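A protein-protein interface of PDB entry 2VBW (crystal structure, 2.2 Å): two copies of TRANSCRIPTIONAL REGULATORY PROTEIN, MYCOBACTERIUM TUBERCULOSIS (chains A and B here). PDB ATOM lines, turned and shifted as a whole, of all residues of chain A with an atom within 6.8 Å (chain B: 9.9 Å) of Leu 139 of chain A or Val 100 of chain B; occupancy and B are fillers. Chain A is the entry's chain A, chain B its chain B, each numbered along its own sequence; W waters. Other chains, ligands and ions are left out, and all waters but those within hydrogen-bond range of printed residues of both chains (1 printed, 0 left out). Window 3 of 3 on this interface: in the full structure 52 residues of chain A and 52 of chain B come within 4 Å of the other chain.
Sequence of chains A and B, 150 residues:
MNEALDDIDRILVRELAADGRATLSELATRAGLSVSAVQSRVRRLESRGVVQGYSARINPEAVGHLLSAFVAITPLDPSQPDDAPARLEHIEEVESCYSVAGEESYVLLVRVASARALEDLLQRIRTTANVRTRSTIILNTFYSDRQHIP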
ATOM      1  N   GLU A  61     -21.494  -9.134 -41.304  1.00  0.00           N
ATOM      2  CA  GLU A  61     -22.698  -8.825 -42.116  1.00  0.00           C
ATOM      3  C   GLU A  61     -22.378  -8.502 -43.572  1.00  0.00           C
ATOM      4  O   GLU A  61     -22.962  -9.111 -44.508  1.00  0.00           O
ATOM      5  CB  GLU A  61     -23.531  -7.707 -41.500  1.00  0.00           C
ATOM      6  CG  GLU A  61     -24.343  -8.164 -40.301  1.00  0.00           C
ATOM      7  CD  GLU A  61     -24.849  -6.998 -39.482  1.00  0.00           C
ATOM      8  OE1 GLU A  61     -24.702  -5.832 -39.951  1.00  0.00           O
ATOM      9  OE2 GLU A  61     -25.379  -7.242 -38.364  1.00  0.00           O
ATOM     10  N   SER A  68     -25.320 -14.729 -36.127  1.00  0.00           N
ATOM     11  CA  SER A  68     -24.276 -15.373 -35.334  1.00  0.00           C
ATOM     12  C   SER A  68     -24.840 -16.034 -34.074  1.00  0.00           C
ATOM     13  O   SER A  68     -25.902 -15.663 -33.605  1.00  0.00           O
ATOM     14  CB  SER A  68     -23.257 -14.348 -34.939  1.00  0.00           C
ATOM     15  OG  SER A  68     -22.713 -13.837 -36.101  1.00  0.00           O
ATOM     16  N   PHE A  70     -23.857 -18.432 -30.242  1.00  0.00           N
ATOM     17  CA  PHE A  70     -23.092 -19.330 -29.396  1.00  0.00           C
ATOM     18  C   PHE A  70     -23.780 -20.668 -29.410  1.00  0.00           C
ATOM     19  O   PHE A  70     -24.983 -20.721 -29.247  1.00  0.00           O
ATOM     20  CB  PHE A  70     -23.010 -18.784 -27.981  1.00  0.00           C
ATOM     21  CG  PHE A  70     -22.148 -17.568 -27.876  1.00  0.00           C
ATOM     22  CD1 PHE A  70     -22.702 -16.314 -27.640  1.00  0.00           C
ATOM     23  CD2 PHE A  70     -20.764 -17.679 -28.006  1.00  0.00           C
ATOM     24  CE1 PHE A  70     -21.894 -15.178 -27.544  1.00  0.00           C
ATOM     25  CE2 PHE A  70     -19.931 -16.546 -27.895  1.00  0.00           C
ATOM     26  CZ  PHE A  70     -20.490 -15.294 -27.656  1.00  0.00           C
ATOM     27  N   THR A 136     -27.504 -20.133 -28.442  1.00  0.00           N
ATOM     28  CA  THR A 136     -27.861 -18.800 -28.003  1.00  0.00           C
ATOM     29  C   THR A 136     -27.553 -17.847 -29.118  1.00  0.00           C
ATOM     30  O   THR A 136     -26.378 -17.542 -29.394  1.00  0.00           O
ATOM     31  CB  THR A 136     -27.026 -18.393 -26.750  1.00  0.00           C
ATOM     32  OG1 THR A 136     -27.233 -19.376 -25.740  1.00  0.00           O
ATOM     33  CG2 THR A 136     -27.427 -17.014 -26.216  1.00  0.00           C
ATOM     34  N   ILE A 137     -28.607 -17.294 -29.686  1.00  0.00           N
ATOM     35  CA  ILE A 137     -28.480 -16.359 -30.779  1.00  0.00           C
ATOM     36  C   ILE A 137     -28.024 -14.941 -30.379  1.00  0.00           C
ATOM     37  O   ILE A 137     -28.525 -14.351 -29.413  1.00  0.00           O
ATOM     38  CB  ILE A 137     -29.764 -16.394 -31.630  1.00  0.00           C
ATOM     39  CG1 ILE A 137     -29.759 -17.739 -32.427  1.00  0.00           C
ATOM     40  CG2 ILE A 137     -29.847 -15.176 -32.542  1.00  0.00           C
ATOM     41  CD1 ILE A 137     -30.944 -18.014 -33.311  1.00  0.00           C
ATOM     42  N   ILE A 138     -27.034 -14.414 -31.124  1.00  0.00           N
ATOM     43  CA  ILE A 138     -26.547 -13.108 -30.885  1.00  0.00           C
ATOM     44  C   ILE A 138     -27.439 -12.109 -31.603  1.00  0.00           C
ATOM     45  O   ILE A 138     -27.699 -12.251 -32.780  1.00  0.00           O
ATOM     46  CB  ILE A 138     -25.073 -12.970 -31.346  1.00  0.00           C
ATOM     47  CG1 ILE A 138     -24.185 -13.860 -30.465  1.00  0.00           C
ATOM     48  CG2 ILE A 138     -24.675 -11.438 -31.349  1.00  0.00           C
ATOM     49  CD1 ILE A 138     -22.786 -14.186 -31.081  1.00  0.00           C
ATOM     50  N   LEU A 139     -27.917 -11.103 -30.895  1.00  0.00           N
ATOM     51  CA  LEU A 139     -28.780 -10.073 -31.500  1.00  0.00           C
ATOM     52  C   LEU A 139     -28.005  -8.862 -31.981  1.00  0.00           C
ATOM     53  O   LEU A 139     -28.394  -8.251 -32.963  1.00  0.00           O
ATOM     54  CB  LEU A 139     -29.898  -9.638 -30.535  1.00  0.00           C
ATOM     55  CG  LEU A 139     -30.717 -10.820 -29.991  1.00  0.00           C
ATOM     56  CD1 LEU A 139     -31.712 -10.380 -28.921  1.00  0.00           C
ATOM     57  CD2 LEU A 139     -31.401 -11.598 -31.101  1.00  0.00           C
ATOM     58  N   ASN A 140     -26.939  -8.493 -31.277  1.00  0.00           N
ATOM     59  CA  ASN A 140     -26.103  -7.361 -31.637  1.00  0.00           C
ATOM     60  C   ASN A 140     -24.759  -7.500 -30.982  1.00  0.00           C
ATOM     61  O   ASN A 140     -24.671  -7.978 -29.853  1.00  0.00           O
ATOM     62  CB  ASN A 140     -26.759  -6.065 -31.161  1.00  0.00           C
ATOM     63  CG  ASN A 140     -26.118  -4.839 -31.755  1.00  0.00           C
ATOM     64  OD1 ASN A 140     -25.802  -4.794 -32.941  1.00  0.00           O
ATOM     65  ND2 ASN A 140     -25.903  -3.847 -30.935  1.00  0.00           N
ATOM     66  N   THR A 141     -23.706  -7.111 -31.701  1.00  0.00           N
ATOM     67  CA  THR A 141     -22.320  -7.096 -31.189  1.00  0.00           C
ATOM     68  C   THR A 141     -21.997  -5.647 -30.855  1.00  0.00           C
ATOM     69  O   THR A 141     -21.894  -4.836 -31.762  1.00  0.00           O
ATOM     70  CB  THR A 141     -21.341  -7.564 -32.258  1.00  0.00           C
ATOM     71  OG1 THR A 141     -21.667  -8.905 -32.649  1.00  0.00           O
ATOM     72  CG2 THR A 141     -19.857  -7.574 -31.733  1.00  0.00           C
ATOM     73  N   PHE A 142     -21.882  -5.281 -29.579  1.00  0.00           N
ATOM     74  CA  PHE A 142     -21.581  -3.886 -29.243  1.00  0.00           C
ATOM     75  C   PHE A 142     -20.149  -3.496 -29.510  1.00  0.00           C
ATOM     76  O   PHE A 142     -19.905  -2.405 -29.941  1.00  0.00           O
ATOM     77  CB  PHE A 142     -21.981  -3.565 -27.820  1.00  0.00           C
ATOM     78  CG  PHE A 142     -23.442  -3.578 -27.646  1.00  0.00           C
ATOM     79  CD1 PHE A 142     -24.184  -2.390 -27.831  1.00  0.00           C
ATOM     80  CD2 PHE A 142     -24.109  -4.785 -27.367  1.00  0.00           C
ATOM     81  CE1 PHE A 142     -25.592  -2.429 -27.720  1.00  0.00           C
ATOM     82  CE2 PHE A 142     -25.483  -4.827 -27.247  1.00  0.00           C
ATOM     83  CZ  PHE A 142     -26.241  -3.681 -27.424  1.00  0.00           C
ATOM     84  N   PHE B  70     -16.595 -16.397 -20.093  1.00  0.00           N
ATOM     85  CA  PHE B  70     -17.805 -15.719 -20.550  1.00  0.00           C
ATOM     86  C   PHE B  70     -18.587 -15.317 -19.345  1.00  0.00           C
ATOM     87  O   PHE B  70     -18.751 -16.100 -18.461  1.00  0.00           O
ATOM     88  CB  PHE B  70     -18.702 -16.629 -21.386  1.00  0.00           C
ATOM     89  CG  PHE B  70     -18.055 -17.108 -22.686  1.00  0.00           C
ATOM     90  CD1 PHE B  70     -17.534 -18.402 -22.775  1.00  0.00           C
ATOM     91  CD2 PHE B  70     -17.957 -16.264 -23.796  1.00  0.00           C
ATOM     92  CE1 PHE B  70     -16.959 -18.856 -23.936  1.00  0.00           C
ATOM     93  CE2 PHE B  70     -17.380 -16.744 -25.006  1.00  0.00           C
ATOM     94  CZ  PHE B  70     -16.879 -18.043 -25.048  1.00  0.00           C
ATOM     95  N   VAL B  71     -19.174 -14.137 -19.348  1.00  0.00           N
ATOM     96  CA  VAL B  71     -19.849 -13.618 -18.195  1.00  0.00           C
ATOM     97  C   VAL B  71     -21.189 -13.184 -18.772  1.00  0.00           C
ATOM     98  O   VAL B  71     -21.200 -12.245 -19.576  1.00  0.00           O
ATOM     99  CB  VAL B  71     -19.118 -12.374 -17.608  1.00  0.00           C
ATOM    100  CG1 VAL B  71     -19.884 -11.858 -16.354  1.00  0.00           C
ATOM    101  CG2 VAL B  71     -17.623 -12.754 -17.156  1.00  0.00           C
ATOM    102  N   ALA B  72     -22.276 -13.865 -18.379  1.00  0.00           N
ATOM    103  CA  ALA B  72     -23.620 -13.584 -18.826  1.00  0.00           C
ATOM    104  C   ALA B  72     -24.191 -12.616 -17.825  1.00  0.00           C
ATOM    105  O   ALA B  72     -24.139 -12.854 -16.618  1.00  0.00           O
ATOM    106  CB  ALA B  72     -24.500 -14.880 -18.851  1.00  0.00           C
ATOM    107  N   ILE B  73     -24.736 -11.511 -18.288  1.00  0.00           N
ATOM    108  CA  ILE B  73     -25.222 -10.520 -17.303  1.00  0.00           C
ATOM    109  C   ILE B  73     -26.676 -10.107 -17.588  1.00  0.00           C
ATOM    110  O   ILE B  73     -27.117 -10.135 -18.722  1.00  0.00           O
ATOM    111  CB  ILE B  73     -24.346  -9.208 -17.255  1.00  0.00           C
ATOM    112  CG1 ILE B  73     -24.290  -8.549 -18.620  1.00  0.00           C
ATOM    113  CG2 ILE B  73     -22.904  -9.450 -16.757  1.00  0.00           C
ATOM    114  CD1 ILE B  73     -23.699  -7.191 -18.581  1.00  0.00           C
ATOM    115  N   THR B  74     -27.418  -9.717 -16.557  1.00  0.00           N
ATOM    116  CA  THR B  74     -28.757  -9.231 -16.736  1.00  0.00           C
ATOM    117  C   THR B  74     -28.991  -8.077 -15.762  1.00  0.00           C
ATOM    118  O   THR B  74     -28.692  -8.203 -14.591  1.00  0.00           O
ATOM    119  CB  THR B  74     -29.781 -10.334 -16.374  1.00  0.00           C
ATOM    120  OG1 THR B  74     -29.614 -11.419 -17.282  1.00  0.00           O
ATOM    121  CG2 THR B  74     -31.237  -9.810 -16.475  1.00  0.00           C
ATOM    122  N   PRO B  75     -29.553  -6.959 -16.257  1.00  0.00           N
ATOM    123  CA  PRO B  75     -29.907  -5.806 -15.400  1.00  0.00           C
ATOM    124  C   PRO B  75     -30.787  -6.182 -14.241  1.00  0.00           C
ATOM    125  O   PRO B  75     -31.713  -6.968 -14.402  1.00  0.00           O
ATOM    126  CB  PRO B  75     -30.620  -4.848 -16.372  1.00  0.00           C
ATOM    127  CG  PRO B  75     -29.859  -5.182 -17.746  1.00  0.00           C
ATOM    128  CD  PRO B  75     -29.892  -6.702 -17.676  1.00  0.00           C
ATOM    129  N   ASP B  82     -31.594   0.476 -20.007  1.00  0.00           N
ATOM    130  CA  ASP B  82     -30.656  -0.594 -20.151  1.00  0.00           C
ATOM    131  C   ASP B  82     -29.452  -0.125 -20.974  1.00  0.00           C
ATOM    132  O   ASP B  82     -29.472  -0.168 -22.190  1.00  0.00           O
ATOM    133  CB  ASP B  82     -31.369  -1.787 -20.792  1.00  0.00           C
ATOM    134  CG  ASP B  82     -30.537  -3.032 -20.764  1.00  0.00           C
ATOM    135  OD1 ASP B  82     -29.379  -2.961 -20.249  1.00  0.00           O
ATOM    136  OD2 ASP B  82     -31.038  -4.042 -21.288  1.00  0.00           O
ATOM    137  N   PRO B  85     -23.909  -2.044 -21.926  1.00  0.00           N
ATOM    138  CA  PRO B  85     -22.694  -2.011 -22.804  1.00  0.00           C
ATOM    139  C   PRO B  85     -21.863  -0.705 -22.747  1.00  0.00           C
ATOM    140  O   PRO B  85     -20.611  -0.768 -22.621  1.00  0.00           O
ATOM    141  CB  PRO B  85     -23.261  -2.206 -24.230  1.00  0.00           C
ATOM    142  CG  PRO B  85     -24.615  -2.862 -24.029  1.00  0.00           C
ATOM    143  CD  PRO B  85     -25.129  -2.386 -22.688  1.00  0.00           C
ATOM    144  N   CYS B  97     -18.708  -7.603 -26.014  1.00  0.00           N
ATOM    145  CA  CYS B  97     -20.030  -7.523 -25.411  1.00  0.00           C
ATOM    146  C   CYS B  97     -21.103  -7.754 -26.474  1.00  0.00           C
ATOM    147  O   CYS B  97     -21.105  -7.117 -27.508  1.00  0.00           O
ATOM    148  CB  CYS B  97     -20.192  -6.146 -24.767  1.00  0.00           C
ATOM    149  SG  CYS B  97     -21.729  -5.844 -24.046  1.00  0.00           S
ATOM    150  N   TYR B  98     -22.026  -8.668 -26.214  1.00  0.00           N
ATOM    151  CA  TYR B  98     -23.085  -9.046 -27.173  1.00  0.00           C
ATOM    152  C   TYR B  98     -24.401  -9.032 -26.445  1.00  0.00           C
ATOM    153  O   TYR B  98     -24.441  -9.489 -25.309  1.00  0.00           O
ATOM    154  CB  TYR B  98     -22.877 -10.505 -27.636  1.00  0.00           C
ATOM    155  CG  TYR B  98     -21.519 -10.836 -28.215  1.00  0.00           C
ATOM    156  CD1 TYR B  98     -20.476 -11.336 -27.396  1.00  0.00           C
ATOM    157  CD2 TYR B  98     -21.288 -10.746 -29.604  1.00  0.00           C
ATOM    158  CE1 TYR B  98     -19.236 -11.686 -27.930  1.00  0.00           C
ATOM    159  CE2 TYR B  98     -20.002 -11.066 -30.166  1.00  0.00           C
ATOM    160  CZ  TYR B  98     -18.994 -11.516 -29.305  1.00  0.00           C
ATOM    161  OH  TYR B  98     -17.778 -11.888 -29.803  1.00  0.00           O
ATOM    162  N   SER B  99     -25.490  -8.564 -27.069  1.00  0.00           N
ATOM    163  CA  SER B  99     -26.806  -8.893 -26.575  1.00  0.00           C
ATOM    164  C   SER B  99     -27.230 -10.200 -27.235  1.00  0.00           C
ATOM    165  O   SER B  99     -26.814 -10.542 -28.341  1.00  0.00           O
ATOM    166  CB  SER B  99     -27.827  -7.794 -26.854  1.00  0.00           C
ATOM    167  OG  SER B  99     -27.846  -7.540 -28.217  1.00  0.00           O
ATOM    168  N   VAL B 100     -28.067 -10.944 -26.547  1.00  0.00           N
ATOM    169  CA  VAL B 100     -28.239 -12.333 -26.921  1.00  0.00           C
ATOM    170  C   VAL B 100     -29.716 -12.687 -26.654  1.00  0.00           C
ATOM    171  O   VAL B 100     -30.379 -12.022 -25.840  1.00  0.00           O
ATOM    172  CB  VAL B 100     -27.160 -13.045 -26.069  1.00  0.00           C
ATOM    173  CG1 VAL B 100     -27.635 -13.665 -24.759  1.00  0.00           C
ATOM    174  CG2 VAL B 100     -25.974 -13.615 -26.876  1.00  0.00           C
ATOM    175  N   ALA B 101     -30.259 -13.632 -27.419  1.00  0.00           N
ATOM    176  CA  ALA B 101     -31.578 -14.199 -27.075  1.00  0.00           C
ATOM    177  C   ALA B 101     -31.334 -15.470 -26.315  1.00  0.00           C
ATOM    178  O   ALA B 101     -31.118 -16.474 -26.918  1.00  0.00           O
ATOM    179  CB  ALA B 101     -32.410 -14.493 -28.327  1.00  0.00           C
ATOM    180  N   GLY B 102     -31.344 -15.444 -24.995  1.00  0.00           N
ATOM    181  CA  GLY B 102     -31.053 -16.680 -24.235  1.00  0.00           C
ATOM    182  C   GLY B 102     -31.675 -16.524 -22.867  1.00  0.00           C
ATOM    183  O   GLY B 102     -32.798 -16.024 -22.750  1.00  0.00           O
ATOM    184  N   GLU B 103     -30.929 -16.913 -21.844  1.00  0.00           N
ATOM    185  CA  GLU B 103     -31.374 -16.793 -20.442  1.00  0.00           C
ATOM    186  C   GLU B 103     -30.974 -15.467 -19.836  1.00  0.00           C
ATOM    187  O   GLU B 103     -31.510 -15.069 -18.856  1.00  0.00           O
ATOM    188  CB  GLU B 103     -30.732 -17.880 -19.571  1.00  0.00           C
ATOM    189  CG  GLU B 103     -31.063 -19.254 -20.079  1.00  0.00           C
ATOM    190  CD  GLU B 103     -31.089 -20.347 -19.004  1.00  0.00           C
ATOM    191  OE1 GLU B 103     -30.762 -20.115 -17.799  1.00  0.00           O
ATOM    192  OE2 GLU B 103     -31.460 -21.473 -19.419  1.00  0.00           O
ATOM    193  N   GLU B 104     -29.982 -14.821 -20.409  1.00  0.00           N
ATOM    194  CA  GLU B 104     -29.403 -13.599 -19.855  1.00  0.00           C
ATOM    195  C   GLU B 104     -29.516 -12.573 -20.957  1.00  0.00           C
ATOM    196  O   GLU B 104     -29.799 -12.954 -22.100  1.00  0.00           O
ATOM    197  CB  GLU B 104     -27.957 -13.870 -19.404  1.00  0.00           C
ATOM    198  CG  GLU B 104     -27.862 -15.009 -18.296  1.00  0.00           C
ATOM    199  CD  GLU B 104     -28.496 -14.564 -16.895  1.00  0.00           C
ATOM    200  OE1 GLU B 104     -28.655 -13.336 -16.650  1.00  0.00           O
ATOM    201  OE2 GLU B 104     -28.776 -15.435 -16.022  1.00  0.00           O
ATOM    202  N   SER B 105     -29.337 -11.299 -20.638  1.00  0.00           N
ATOM    203  CA  SER B 105     -29.409 -10.265 -21.623  1.00  0.00           C
ATOM    204  C   SER B 105     -28.152 -10.085 -22.456  1.00  0.00           C
ATOM    205  O   SER B 105     -28.253  -9.723 -23.605  1.00  0.00           O
ATOM    206  CB  SER B 105     -29.757  -8.915 -20.943  1.00  0.00           C
ATOM    207  OG  SER B 105     -31.032  -9.095 -20.361  1.00  0.00           O
ATOM    208  N   TYR B 106     -26.970 -10.229 -21.852  1.00  0.00           N
ATOM    209  CA  TYR B 106     -25.726  -9.961 -22.610  1.00  0.00           C
ATOM    210  C   TYR B 106     -24.770 -11.047 -22.219  1.00  0.00           C
ATOM    211  O   TYR B 106     -24.834 -11.545 -21.110  1.00  0.00           O
ATOM    212  CB  TYR B 106     -25.059  -8.613 -22.245  1.00  0.00           C
ATOM    213  CG  TYR B 106     -25.962  -7.414 -22.364  1.00  0.00           C
ATOM    214  CD1 TYR B 106     -26.122  -6.770 -23.587  1.00  0.00           C
ATOM    215  CD2 TYR B 106     -26.705  -6.961 -21.258  1.00  0.00           C
ATOM    216  CE1 TYR B 106     -26.974  -5.698 -23.729  1.00  0.00           C
ATOM    217  CE2 TYR B 106     -27.578  -5.868 -21.387  1.00  0.00           C
ATOM    218  CZ  TYR B 106     -27.676  -5.239 -22.654  1.00  0.00           C
ATOM    219  OH  TYR B 106     -28.510  -4.176 -22.852  1.00  0.00           O
ATOM    220  N   VAL B 107     -23.806 -11.286 -23.091  1.00  0.00           N
ATOM    221  CA  VAL B 107     -22.644 -12.111 -22.802  1.00  0.00           C
ATOM    222  C   VAL B 107     -21.398 -11.261 -23.079  1.00  0.00           C
ATOM    223  O   VAL B 107     -21.336 -10.586 -24.110  1.00  0.00           O
ATOM    224  CB  VAL B 107     -22.642 -13.365 -23.727  1.00  0.00           C
ATOM    225  CG1 VAL B 107     -21.317 -14.171 -23.583  1.00  0.00           C
ATOM    226  CG2 VAL B 107     -23.863 -14.217 -23.453  1.00  0.00           C
ATOM    227  N   LEU B 108     -20.440 -11.292 -22.144  1.00  0.00           N
ATOM    228  CA  LEU B 108     -19.117 -10.658 -22.215  1.00  0.00           C
ATOM    229  C   LEU B 108     -18.056 -11.718 -22.297  1.00  0.00           C
ATOM    230  O   LEU B 108     -18.182 -12.782 -21.687  1.00  0.00           O
ATOM    231  CB  LEU B 108     -18.770  -9.900 -20.904  1.00  0.00           C
ATOM    232  CG  LEU B 108     -19.831  -8.989 -20.278  1.00  0.00           C
ATOM    233  CD1 LEU B 108     -19.368  -8.256 -18.999  1.00  0.00           C
ATOM    234  CD2 LEU B 108     -20.317  -7.998 -21.324  1.00  0.00           C
ATOM    235  N   ARG B 134     -23.199 -14.193 -14.275  1.00  0.00           N
ATOM    236  CA  ARG B 134     -23.077 -15.604 -14.266  1.00  0.00           C
ATOM    237  C   ARG B 134     -21.909 -15.991 -15.203  1.00  0.00           C
ATOM    238  O   ARG B 134     -21.958 -15.782 -16.425  1.00  0.00           O
ATOM    239  CB  ARG B 134     -24.400 -16.293 -14.621  1.00  0.00           C
ATOM    240  CG  ARG B 134     -24.174 -17.654 -15.177  1.00  0.00           C
ATOM    241  CD  ARG B 134     -25.277 -18.634 -14.876  1.00  0.00           C
ATOM    242  NE  ARG B 134     -26.504 -18.483 -15.653  1.00  0.00           N
ATOM    243  CZ  ARG B 134     -26.616 -18.599 -16.987  1.00  0.00           C
ATOM    244  NH1 ARG B 134     -25.536 -18.820 -17.783  1.00  0.00           N
ATOM    245  NH2 ARG B 134     -27.829 -18.442 -17.541  1.00  0.00           N
HETATM  246  O   HOH W   1     -28.226 -18.524 -22.646  1.00  0.00           O
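O of Ile 137 of chain A lies within hydrogen-bond range of N of Ala 101 of chain B.
The backbone carbonyl oxygen (O) of Cys 97 of chain B is in hydrogen-bond range of the backbone NH (N) of Phe 142 of chain A (2.9 Å).
The backbone NH (N) of Ser 99 of chain B is in hydrogen-bond range of the backbone carbonyl oxygen (O) of Asn 140 of chain A (3.0 Å).
The backbone NH of Leu 139 of chain A sits at hydrogen-bond distance from the backbone carbonyl oxygen of Ser 99 of chain B, at 2.8 Å.
The backbone carbonyl oxygen (O) of Phe 70 of chain A lies within hydrogen-bond range of the backbone NH (N) of Thr 136 of chain A, 2.7 Å away.
The backbone carbonyl oxygen (O) of Ser 68 of chain A sits at hydrogen-bond distance from the backbone NH (N) of Ile 138 of chain A (3.0 Å).
N of Val 100 of chain B sits at hydrogen-bond distance from O of Ser 105 of chain B (3.2 Å).
The side-chain hydroxyl of Tyr 106 of chain B is in hydrogen-bond range of the side-chain carboxylate of Asp 82 of chain B, at 3.0 Å.
O of Tyr 98 of chain B sits at hydrogen-bond distance from N of Val 107 of chain B (2.9 Å).
N of Ile 73 of chain B sits at hydrogen-bond distance from O of Tyr 106 of chain B.
Phe 70 of chain B touches Phe 70 of chain A.
Phe 70 of chain A touches Tyr 98 of chain B.
Ile 138 of chain A touches Ser 99 of chain B (CA to O, 3.6 Å).
O of Val 100 of chain B touches CD1 of Leu 139 of chain A, 3.7 Å away.
Leu 139 of chain A touches Ala 101 of chain B.
Asn 140 of chain A touches Tyr 98 of chain B (O to CA, 3.3 Å).
Thr 141 of chain A touches Cys 97 of chain B (C to O, 3.8 Å).
Thr 141 of chain A touches Tyr 98 of chain B.
Ser 99 of chain B touches Phe 142 of chain A.
Phe 142 of chain A touches Tyr 106 of chain B.
Printed residues of chain B within 4 Å of Ile 138 of chain A: Tyr 98 and Ser 99.
Leu 139 of chain A touches just these residues of chain B: Ser 99, Val 100 and Ala 101.
Asn 140 of chain A touches two residues of chain B.
Printed residues of chain B within 4 Å of Thr 141 of chain A: Cys 97 and Tyr 98.
Printed residues of chain B within 4 Å of Phe 142 of chain A: Pro 85, Cys 97, Ser 99 and Tyr 106.
Asp 82 of chain B touches none of the printed residues of chain A.
Of the printed residues of chain A, Cys 97 of chain B touches Thr 141 and Phe 142.
Of the printed residues of chain A, Val 100 of chain B touches Thr 136, Ile 137 and Leu 139.
Of the printed residues of chain A, Ala 101 of chain B touches Thr 136 (3.8 Å), Ile 137 (2.7 Å) and Leu 139 (3.8 Å).
The nearest residue of chain B that does not touch Leu 139 of chain A is Tyr 98 of chain B (6.0 Å).
The nearest printed residue of chain A that does not touch Ser 99 of chain B is Ile 137 of chain A (4.3 Å).
Of the 10 printed residues of chain A, 8 touch a printed residue of chain B.
Of the 21 printed residues of chain B, 8 touch a printed residue of chain A.
Hydrophobic or aromatic side chains of chain B within 4 Å of the printed part of chain A: Phe 70, Pro 85, Tyr 98, Val 100 and Tyr 106.
Among the printed residues, 19 pairs touch across the chains.
Among the printed residues, no Asp or Glu carboxylate lies within 4 Å of a Lys or Arg side-chain nitrogen of the other chain.
Phe 70 of chain B touches its own counterpart, Phe 70 of chain A.
Of the 19 pairs that touch across the chains among the printed residues, 1 has its exchanged pair printed and touching as well.
Water W1 bridges N of Glu 103 of chain B (3.2 Å) and OG1 of Thr 136 of chain A (3.4 Å).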
